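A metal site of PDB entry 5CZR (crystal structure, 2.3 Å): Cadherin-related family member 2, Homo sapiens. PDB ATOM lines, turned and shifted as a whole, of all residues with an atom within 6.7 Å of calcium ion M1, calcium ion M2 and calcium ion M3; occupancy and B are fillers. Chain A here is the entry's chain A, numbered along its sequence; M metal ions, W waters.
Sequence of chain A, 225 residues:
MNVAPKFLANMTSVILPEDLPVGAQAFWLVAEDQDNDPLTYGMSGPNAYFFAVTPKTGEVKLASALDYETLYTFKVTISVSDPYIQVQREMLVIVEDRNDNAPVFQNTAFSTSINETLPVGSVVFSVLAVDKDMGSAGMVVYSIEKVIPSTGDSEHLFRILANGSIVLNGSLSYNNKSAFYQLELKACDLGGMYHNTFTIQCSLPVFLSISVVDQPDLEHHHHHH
Calcium ion M2 is bound by OD1 of Asp 97 (2.2 Å), OD1 of Asp 133 (2.3 Å), OD1 of Asp 100 (2.3 Å), OE1 of Glu 18 (2.3 Å), OE2 of Glu 69 (2.4 Å) and O of Arg 98 (2.4 Å).
Slightly farther from calcium ion M2 lies OE1 of Glu 69 (2.9 Å).
Calcium ion M1 is bound by the backbone carbonyl oxygen (O) of Asn 101 (2.2 Å), the side-chain amide oxygen (OD1) of Asn 99 (2.3 Å), the backbone carbonyl oxygen (O) of Ala 137 (2.3 Å), the side-chain carboxylate (OD2) of Asp 189 (2.5 Å), the side-chain carboxylate (OD2) of Asp 133 (2.5 Å), the side-chain carboxylate (OD2) of Asp 131 (2.5 Å) and the side-chain carboxylate (OD1) of Asp 131 (2.6 Å).
Calcium ion M1 has seven donor atoms within binding distance.
O of Gly 191 is in hydrogen-bond range of N of Ala 137, 3.3 Å away.
The backbone NH of Tyr 68 sits close to the side-chain carboxylate of Glu 18, 3.0 Å away.
O of Asn 99 is in hydrogen-bond range of NE2 of Gln 201, at 2.8 Å.
The backbone NH of Glu 18 is in hydrogen-bond range of the backbone carbonyl oxygen of Glu 96 (3.0 Å).
OE1 of Glu 69 sits close to ND2 of Asn 101 (3.4 Å).
OD2 of Asp 67 is in hydrogen-bond range of OG1 of Thr 70, at 3.2 Å.
The side-chain carboxylate (OD1) of Asp 189 sits at hydrogen-bond distance from the backbone NH (N) of Gly 191, at 2.9 Å.
OE1 of Glu 96 is in salt-bridge range of NH2 of Arg 98 (2.9 Å).
Of the 26 residues printed, 6 come within 4 Å of calcium ion M1.
Within 4 Å of calcium ion M2: Glu 18, Glu 69, Asp 97, Arg 98, Asp 100, Asn 101 and Asp 133.
Along chain A the residues within 4 Å of calcium ion M2 span positions 18 to 133.
Four residues have an atom within 4 Å of calcium ion M3: Glu 18, Asp 67, Glu 69 and Asp 100.
The nearest printed residue that does not touch calcium ion M3 is Tyr 68 (4.1 Å).
Calcium ion M3 is bound by OD1 of Asp 67, at 2.1 Å.
Calcium ion M3 is bound by water W1 (2.2 Å).
Water W2 is bound to calcium ion M3, at 2.2 Å.
Calcium ion M3 is bound by OE1 of Glu 69 (2.2 Å).
OD2 of Asp 100 is bound to calcium ion M3 (2.3 Å).
Calcium ion M3 is bound by OE2 of Glu 18 (2.3 Å).
Calcium ion M3 has six donor atoms within binding distance.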
ATOM      1  N   GLU A  18      12.110 -30.842  13.430  1.00  0.00           N
ATOM      2  CA  GLU A  18      11.016 -31.731  13.034  1.00  0.00           C
ATOM      3  C   GLU A  18      11.290 -32.440  11.690  1.00  0.00           C
ATOM      4  O   GLU A  18      10.733 -33.490  11.450  1.00  0.00           O
ATOM      5  CB  GLU A  18       9.655 -31.012  12.997  1.00  0.00           C
ATOM      6  CG  GLU A  18       9.530 -29.908  11.949  1.00  0.00           C
ATOM      7  CD  GLU A  18       8.096 -29.520  11.657  1.00  0.00           C
ATOM      8  OE1 GLU A  18       7.855 -28.327  11.423  1.00  0.00           O
ATOM      9  OE2 GLU A  18       7.221 -30.417  11.654  1.00  0.00           O
ATOM     10  N   LEU A  66       9.452 -37.245  13.235  1.00  0.00           N
ATOM     11  CA  LEU A  66       8.965 -36.176  14.085  1.00  0.00           C
ATOM     12  C   LEU A  66       7.979 -35.308  13.329  1.00  0.00           C
ATOM     13  O   LEU A  66       7.971 -35.314  12.102  1.00  0.00           O
ATOM     14  CB  LEU A  66      10.131 -35.300  14.580  1.00  0.00           C
ATOM     15  CG  LEU A  66      11.273 -36.051  15.301  1.00  0.00           C
ATOM     16  CD1 LEU A  66      12.415 -35.103  15.651  1.00  0.00           C
ATOM     17  CD2 LEU A  66      10.749 -36.712  16.582  1.00  0.00           C
ATOM     18  N   ASP A  67       7.189 -34.527  14.051  1.00  0.00           N
ATOM     19  CA  ASP A  67       6.315 -33.501  13.423  1.00  0.00           C
ATOM     20  C   ASP A  67       5.876 -32.495  14.475  1.00  0.00           C
ATOM     21  O   ASP A  67       5.169 -32.852  15.414  1.00  0.00           O
ATOM     22  CB  ASP A  67       5.100 -34.160  12.752  1.00  0.00           C
ATOM     23  CG  ASP A  67       4.169 -33.177  12.086  1.00  0.00           C
ATOM     24  OD1 ASP A  67       4.503 -31.973  12.001  1.00  0.00           O
ATOM     25  OD2 ASP A  67       3.083 -33.603  11.620  1.00  0.00           O
ATOM     26  N   TYR A  68       6.370 -31.267  14.355  1.00  0.00           N
ATOM     27  CA  TYR A  68       6.047 -30.186  15.295  1.00  0.00           C
ATOM     28  C   TYR A  68       4.542 -29.961  15.360  1.00  0.00           C
ATOM     29  O   TYR A  68       4.012 -29.651  16.420  1.00  0.00           O
ATOM     30  CB  TYR A  68       6.739 -28.882  14.877  1.00  0.00           C
ATOM     31  CG  TYR A  68       6.506 -27.745  15.829  1.00  0.00           C
ATOM     32  CD1 TYR A  68       7.373 -27.517  16.919  1.00  0.00           C
ATOM     33  CD2 TYR A  68       5.442 -26.882  15.647  1.00  0.00           C
ATOM     34  CE1 TYR A  68       7.166 -26.471  17.817  1.00  0.00           C
ATOM     35  CE2 TYR A  68       5.211 -25.825  16.536  1.00  0.00           C
ATOM     36  CZ  TYR A  68       6.073 -25.621  17.608  1.00  0.00           C
ATOM     37  OH  TYR A  68       5.825 -24.590  18.464  1.00  0.00           O
ATOM     38  N   GLU A  69       3.851 -30.149  14.233  1.00  0.00           N
ATOM     39  CA  GLU A  69       2.443 -29.846  14.149  1.00  0.00           C
ATOM     40  C   GLU A  69       1.593 -30.893  14.895  1.00  0.00           C
ATOM     41  O   GLU A  69       0.421 -30.676  15.102  1.00  0.00           O
ATOM     42  CB  GLU A  69       2.003 -29.742  12.673  1.00  0.00           C
ATOM     43  CG  GLU A  69       2.328 -28.404  11.993  1.00  0.00           C
ATOM     44  CD  GLU A  69       3.803 -28.148  11.745  1.00  0.00           C
ATOM     45  OE1 GLU A  69       4.510 -29.022  11.264  1.00  0.00           O
ATOM     46  OE2 GLU A  69       4.300 -27.033  12.006  1.00  0.00           O
ATOM     47  N   THR A  70       2.205 -32.005  15.292  1.00  0.00           N
ATOM     48  CA  THR A  70       1.476 -33.161  15.864  1.00  0.00           C
ATOM     49  C   THR A  70       1.877 -33.427  17.322  1.00  0.00           C
ATOM     50  O   THR A  70       1.025 -33.737  18.134  1.00  0.00           O
ATOM     51  CB  THR A  70       1.725 -34.368  14.975  1.00  0.00           C
ATOM     52  OG1 THR A  70       0.882 -34.237  13.832  1.00  0.00           O
ATOM     53  CG2 THR A  70       1.423 -35.707  15.638  1.00  0.00           C
ATOM     54  N   GLU A  96      11.761 -28.720  17.210  1.00  0.00           N
ATOM     55  CA  GLU A  96      11.735 -27.383  16.590  1.00  0.00           C
ATOM     56  C   GLU A  96      10.909 -27.341  15.311  1.00  0.00           C
ATOM     57  O   GLU A  96      10.968 -28.249  14.476  1.00  0.00           O
ATOM     58  CB  GLU A  96      13.123 -26.896  16.280  1.00  0.00           C
ATOM     59  CG  GLU A  96      13.862 -26.424  17.538  1.00  0.00           C
ATOM     60  CD  GLU A  96      15.114 -25.548  17.301  1.00  0.00           C
ATOM     61  OE1 GLU A  96      15.750 -25.632  16.238  1.00  0.00           O
ATOM     62  OE2 GLU A  96      15.499 -24.808  18.225  1.00  0.00           O
ATOM     63  N   ASP A  97      10.110 -26.287  15.189  1.00  0.00           N
ATOM     64  CA  ASP A  97       9.308 -26.052  14.012  1.00  0.00           C
ATOM     65  C   ASP A  97      10.219 -25.738  12.840  1.00  0.00           C
ATOM     66  O   ASP A  97      11.198 -25.027  12.960  1.00  0.00           O
ATOM     67  CB  ASP A  97       8.329 -24.914  14.261  1.00  0.00           C
ATOM     68  CG  ASP A  97       7.383 -24.683  13.103  1.00  0.00           C
ATOM     69  OD1 ASP A  97       6.861 -25.665  12.499  1.00  0.00           O
ATOM     70  OD2 ASP A  97       7.163 -23.486  12.778  1.00  0.00           O
ATOM     71  N   ARG A  98       9.855 -26.264  11.690  1.00  0.00           N
ATOM     72  CA  ARG A  98      10.502 -25.906  10.455  1.00  0.00           C
ATOM     73  C   ARG A  98       9.408 -25.489   9.464  1.00  0.00           C
ATOM     74  O   ARG A  98       8.204 -25.711   9.707  1.00  0.00           O
ATOM     75  CB  ARG A  98      11.315 -27.102   9.936  1.00  0.00           C
ATOM     76  CG  ARG A  98      12.537 -27.481  10.800  1.00  0.00           C
ATOM     77  CD  ARG A  98      13.627 -26.438  10.594  1.00  0.00           C
ATOM     78  NE  ARG A  98      14.767 -26.488  11.489  1.00  0.00           N
ATOM     79  CZ  ARG A  98      14.876 -25.804  12.615  1.00  0.00           C
ATOM     80  NH1 ARG A  98      13.905 -25.019  13.056  1.00  0.00           N
ATOM     81  NH2 ARG A  98      15.957 -25.940  13.317  1.00  0.00           N
ATOM     82  N   ASN A  99       9.823 -24.891   8.338  1.00  0.00           N
ATOM     83  CA  ASN A  99       8.835 -24.372   7.377  1.00  0.00           C
ATOM     84  C   ASN A  99       8.329 -25.418   6.394  1.00  0.00           C
ATOM     85  O   ASN A  99       8.661 -25.377   5.196  1.00  0.00           O
ATOM     86  CB  ASN A  99       9.378 -23.159   6.644  1.00  0.00           C
ATOM     87  CG  ASN A  99       8.311 -22.447   5.872  1.00  0.00           C
ATOM     88  OD1 ASN A  99       7.135 -22.661   6.117  1.00  0.00           O
ATOM     89  ND2 ASN A  99       8.713 -21.557   4.959  1.00  0.00           N
ATOM     90  N   ASP A 100       7.524 -26.340   6.883  1.00  0.00           N
ATOM     91  CA  ASP A 100       7.068 -27.492   6.107  1.00  0.00           C
ATOM     92  C   ASP A 100       5.582 -27.442   5.708  1.00  0.00           C
ATOM     93  O   ASP A 100       5.066 -28.406   5.135  1.00  0.00           O
ATOM     94  CB  ASP A 100       7.339 -28.791   6.877  1.00  0.00           C
ATOM     95  CG  ASP A 100       6.600 -28.864   8.195  1.00  0.00           C
ATOM     96  OD1 ASP A 100       6.043 -27.831   8.689  1.00  0.00           O
ATOM     97  OD2 ASP A 100       6.563 -29.977   8.748  1.00  0.00           O
ATOM     98  N   ASN A 101       4.917 -26.321   5.991  1.00  0.00           N
ATOM     99  CA  ASN A 101       3.577 -26.074   5.514  1.00  0.00           C
ATOM    100  C   ASN A 101       3.491 -24.820   4.664  1.00  0.00           C
ATOM    101  O   ASN A 101       4.258 -23.850   4.824  1.00  0.00           O
ATOM    102  CB  ASN A 101       2.647 -25.944   6.701  1.00  0.00           C
ATOM    103  CG  ASN A 101       2.461 -27.239   7.447  1.00  0.00           C
ATOM    104  OD1 ASN A 101       1.624 -28.040   7.084  1.00  0.00           O
ATOM    105  ND2 ASN A 101       3.294 -27.481   8.452  1.00  0.00           N
ATOM    106  N   ALA A 102       2.540 -24.856   3.756  1.00  0.00           N
ATOM    107  CA  ALA A 102       2.285 -23.754   2.843  1.00  0.00           C
ATOM    108  C   ALA A 102       0.978 -23.069   3.287  1.00  0.00           C
ATOM    109  O   ALA A 102       0.124 -23.690   3.902  1.00  0.00           O
ATOM    110  CB  ALA A 102       2.128 -24.292   1.427  1.00  0.00           C
ATOM    111  N   PRO A 103       0.799 -21.788   2.942  1.00  0.00           N
ATOM    112  CA  PRO A 103      -0.526 -21.229   3.143  1.00  0.00           C
ATOM    113  C   PRO A 103      -1.636 -21.951   2.343  1.00  0.00           C
ATOM    114  O   PRO A 103      -1.422 -22.349   1.206  1.00  0.00           O
ATOM    115  CB  PRO A 103      -0.361 -19.799   2.669  1.00  0.00           C
ATOM    116  CG  PRO A 103       1.104 -19.518   2.776  1.00  0.00           C
ATOM    117  CD  PRO A 103       1.745 -20.818   2.390  1.00  0.00           C
ATOM    118  N   ASP A 131      -1.474 -20.528   7.344  1.00  0.00           N
ATOM    119  CA  ASP A 131      -0.277 -21.365   7.347  1.00  0.00           C
ATOM    120  C   ASP A 131      -0.037 -21.829   8.768  1.00  0.00           C
ATOM    121  O   ASP A 131       0.096 -21.016   9.678  1.00  0.00           O
ATOM    122  CB  ASP A 131       0.889 -20.519   6.865  1.00  0.00           C
ATOM    123  CG  ASP A 131       2.148 -21.316   6.614  1.00  0.00           C
ATOM    124  OD1 ASP A 131       2.662 -21.968   7.548  1.00  0.00           O
ATOM    125  OD2 ASP A 131       2.688 -21.197   5.500  1.00  0.00           O
ATOM    126  N   LYS A 132       0.064 -23.134   8.961  1.00  0.00           N
ATOM    127  CA  LYS A 132       0.232 -23.727  10.294  1.00  0.00           C
ATOM    128  C   LYS A 132       1.539 -23.433  11.033  1.00  0.00           C
ATOM    129  O   LYS A 132       1.598 -23.561  12.256  1.00  0.00           O
ATOM    130  CB  LYS A 132       0.144 -25.245  10.186  1.00  0.00           C
ATOM    131  CG  LYS A 132      -1.238 -25.745   9.802  1.00  0.00           C
ATOM    132  CD  LYS A 132      -1.149 -27.178   9.308  1.00  0.00           C
ATOM    133  CE  LYS A 132      -2.519 -27.690   8.880  1.00  0.00           C
ATOM    134  NZ  LYS A 132      -2.458 -29.168   8.805  1.00  0.00           N
ATOM    135  N   ASP A 133       2.581 -23.075  10.310  1.00  0.00           N
ATOM    136  CA  ASP A 133       3.890 -22.927  10.920  1.00  0.00           C
ATOM    137  C   ASP A 133       3.926 -21.723  11.850  1.00  0.00           C
ATOM    138  O   ASP A 133       3.024 -20.910  11.832  1.00  0.00           O
ATOM    139  CB  ASP A 133       4.975 -22.841   9.845  1.00  0.00           C
ATOM    140  CG  ASP A 133       5.061 -24.126   9.015  1.00  0.00           C
ATOM    141  OD1 ASP A 133       5.059 -25.226   9.603  1.00  0.00           O
ATOM    142  OD2 ASP A 133       5.102 -24.047   7.776  1.00  0.00           O
ATOM    143  N   MET A 134       4.946 -21.682  12.719  1.00  0.00           N
ATOM    144  CA  MET A 134       5.167 -20.601  13.682  1.00  0.00           C
ATOM    145  C   MET A 134       6.011 -19.463  13.089  1.00  0.00           C
ATOM    146  O   MET A 134       6.758 -19.647  12.147  1.00  0.00           O
ATOM    147  CB  MET A 134       5.880 -21.159  14.929  1.00  0.00           C
ATOM    148  CG  MET A 134       5.090 -22.235  15.699  1.00  0.00           C
ATOM    149  SD  MET A 134       3.511 -21.590  16.314  1.00  0.00           S
ATOM    150  CE  MET A 134       2.917 -23.004  17.219  1.00  0.00           C
ATOM    151  N   SER A 136       7.684 -16.355  11.297  1.00  0.00           N
ATOM    152  CA  SER A 136       7.658 -15.860   9.925  1.00  0.00           C
ATOM    153  C   SER A 136       7.218 -16.949   8.976  1.00  0.00           C
ATOM    154  O   SER A 136       6.625 -16.667   7.923  1.00  0.00           O
ATOM    155  CB  SER A 136       9.032 -15.407   9.480  1.00  0.00           C
ATOM    156  OG  SER A 136       9.436 -14.349  10.311  1.00  0.00           O
ATOM    157  N   ALA A 137       7.529 -18.200   9.343  1.00  0.00           N
ATOM    158  CA  ALA A 137       7.151 -19.329   8.505  1.00  0.00           C
ATOM    159  C   ALA A 137       5.637 -19.527   8.396  1.00  0.00           C
ATOM    160  O   ALA A 137       5.178 -20.273   7.503  1.00  0.00           O
ATOM    161  CB  ALA A 137       7.836 -20.580   9.010  1.00  0.00           C
ATOM    162  N   GLY A 138       4.887 -18.891   9.301  1.00  0.00           N
ATOM    163  CA  GLY A 138       3.447 -18.879   9.290  1.00  0.00           C
ATOM    164  C   GLY A 138       2.774 -17.545   8.927  1.00  0.00           C
ATOM    165  O   GLY A 138       1.546 -17.490   8.902  1.00  0.00           O
ATOM    166  N   MET A 139       3.567 -16.492   8.676  1.00  0.00           N
ATOM    167  CA  MET A 139       3.016 -15.178   8.275  1.00  0.00           C
ATOM    168  C   MET A 139       2.737 -15.196   6.788  1.00  0.00           C
ATOM    169  O   MET A 139       3.585 -15.516   5.970  1.00  0.00           O
ATOM    170  CB  MET A 139       3.953 -14.022   8.642  1.00  0.00           C
ATOM    171  CG  MET A 139       4.041 -13.718  10.149  1.00  0.00           C
ATOM    172  SD  MET A 139       5.176 -12.378  10.652  1.00  0.00           S
ATOM    173  CE  MET A 139       5.444 -12.622  12.430  1.00  0.00           C
ATOM    174  N   ASP A 189       4.374 -17.692   2.600  1.00  0.00           N
ATOM    175  CA  ASP A 189       4.854 -17.320   3.942  1.00  0.00           C
ATOM    176  C   ASP A 189       6.049 -16.425   3.770  1.00  0.00           C
ATOM    177  O   ASP A 189       6.480 -16.203   2.657  1.00  0.00           O
ATOM    178  CB  ASP A 189       5.119 -18.528   4.865  1.00  0.00           C
ATOM    179  CG  ASP A 189       6.079 -19.547   4.283  1.00  0.00           C
ATOM    180  OD1 ASP A 189       7.122 -19.158   3.679  1.00  0.00           O
ATOM    181  OD2 ASP A 189       5.827 -20.761   4.421  1.00  0.00           O
ATOM    182  N   LEU A 190       6.597 -15.898   4.859  1.00  0.00           N
ATOM    183  CA  LEU A 190       7.834 -15.096   4.822  1.00  0.00           C
ATOM    184  C   LEU A 190       9.075 -15.917   4.991  1.00  0.00           C
ATOM    185  O   LEU A 190      10.178 -15.401   5.103  1.00  0.00           O
ATOM    186  CB  LEU A 190       7.797 -14.004   5.900  1.00  0.00           C
ATOM    187  CG  LEU A 190       6.761 -12.905   5.608  1.00  0.00           C
ATOM    188  CD1 LEU A 190       6.641 -11.974   6.800  1.00  0.00           C
ATOM    189  CD2 LEU A 190       7.124 -12.145   4.329  1.00  0.00           C
ATOM    190  N   GLY A 191       8.907 -17.243   5.011  1.00  0.00           N
ATOM    191  CA  GLY A 191      10.054 -18.145   4.974  1.00  0.00           C
ATOM    192  C   GLY A 191      10.586 -18.575   6.336  1.00  0.00           C
ATOM    193  O   GLY A 191      10.185 -18.046   7.389  1.00  0.00           O
ATOM    194  N   GLN A 201       7.373 -21.005   1.310  1.00  0.00           N
ATOM    195  CA  GLN A 201       6.270 -21.857   0.815  1.00  0.00           C
ATOM    196  C   GLN A 201       5.140 -21.029   0.285  1.00  0.00           C
ATOM    197  O   GLN A 201       4.795 -20.022   0.890  1.00  0.00           O
ATOM    198  CB  GLN A 201       5.718 -22.777   1.921  1.00  0.00           C
ATOM    199  CG  GLN A 201       6.765 -23.613   2.627  1.00  0.00           C
ATOM    200  CD  GLN A 201       7.062 -24.919   1.894  1.00  0.00           C
ATOM    201  OE1 GLN A 201       6.655 -25.117   0.758  1.00  0.00           O
ATOM    202  NE2 GLN A 201       7.770 -25.820   2.549  1.00  0.00           N
HETATM  203 CA    CA M   1       4.862 -22.177   6.183  1.00  0.00          CA
HETATM  204 CA    CA M   2       6.285 -26.762  10.733  1.00  0.00          CA
HETATM  205 CA    CA M   3       5.373 -30.900  10.432  1.00  0.00          CA
HETATM  206  O   HOH W   1       3.758 -30.607   9.006  1.00  0.00           O
HETATM  207  O   HOH W   2       6.187 -32.826   9.681  1.00  0.00           O
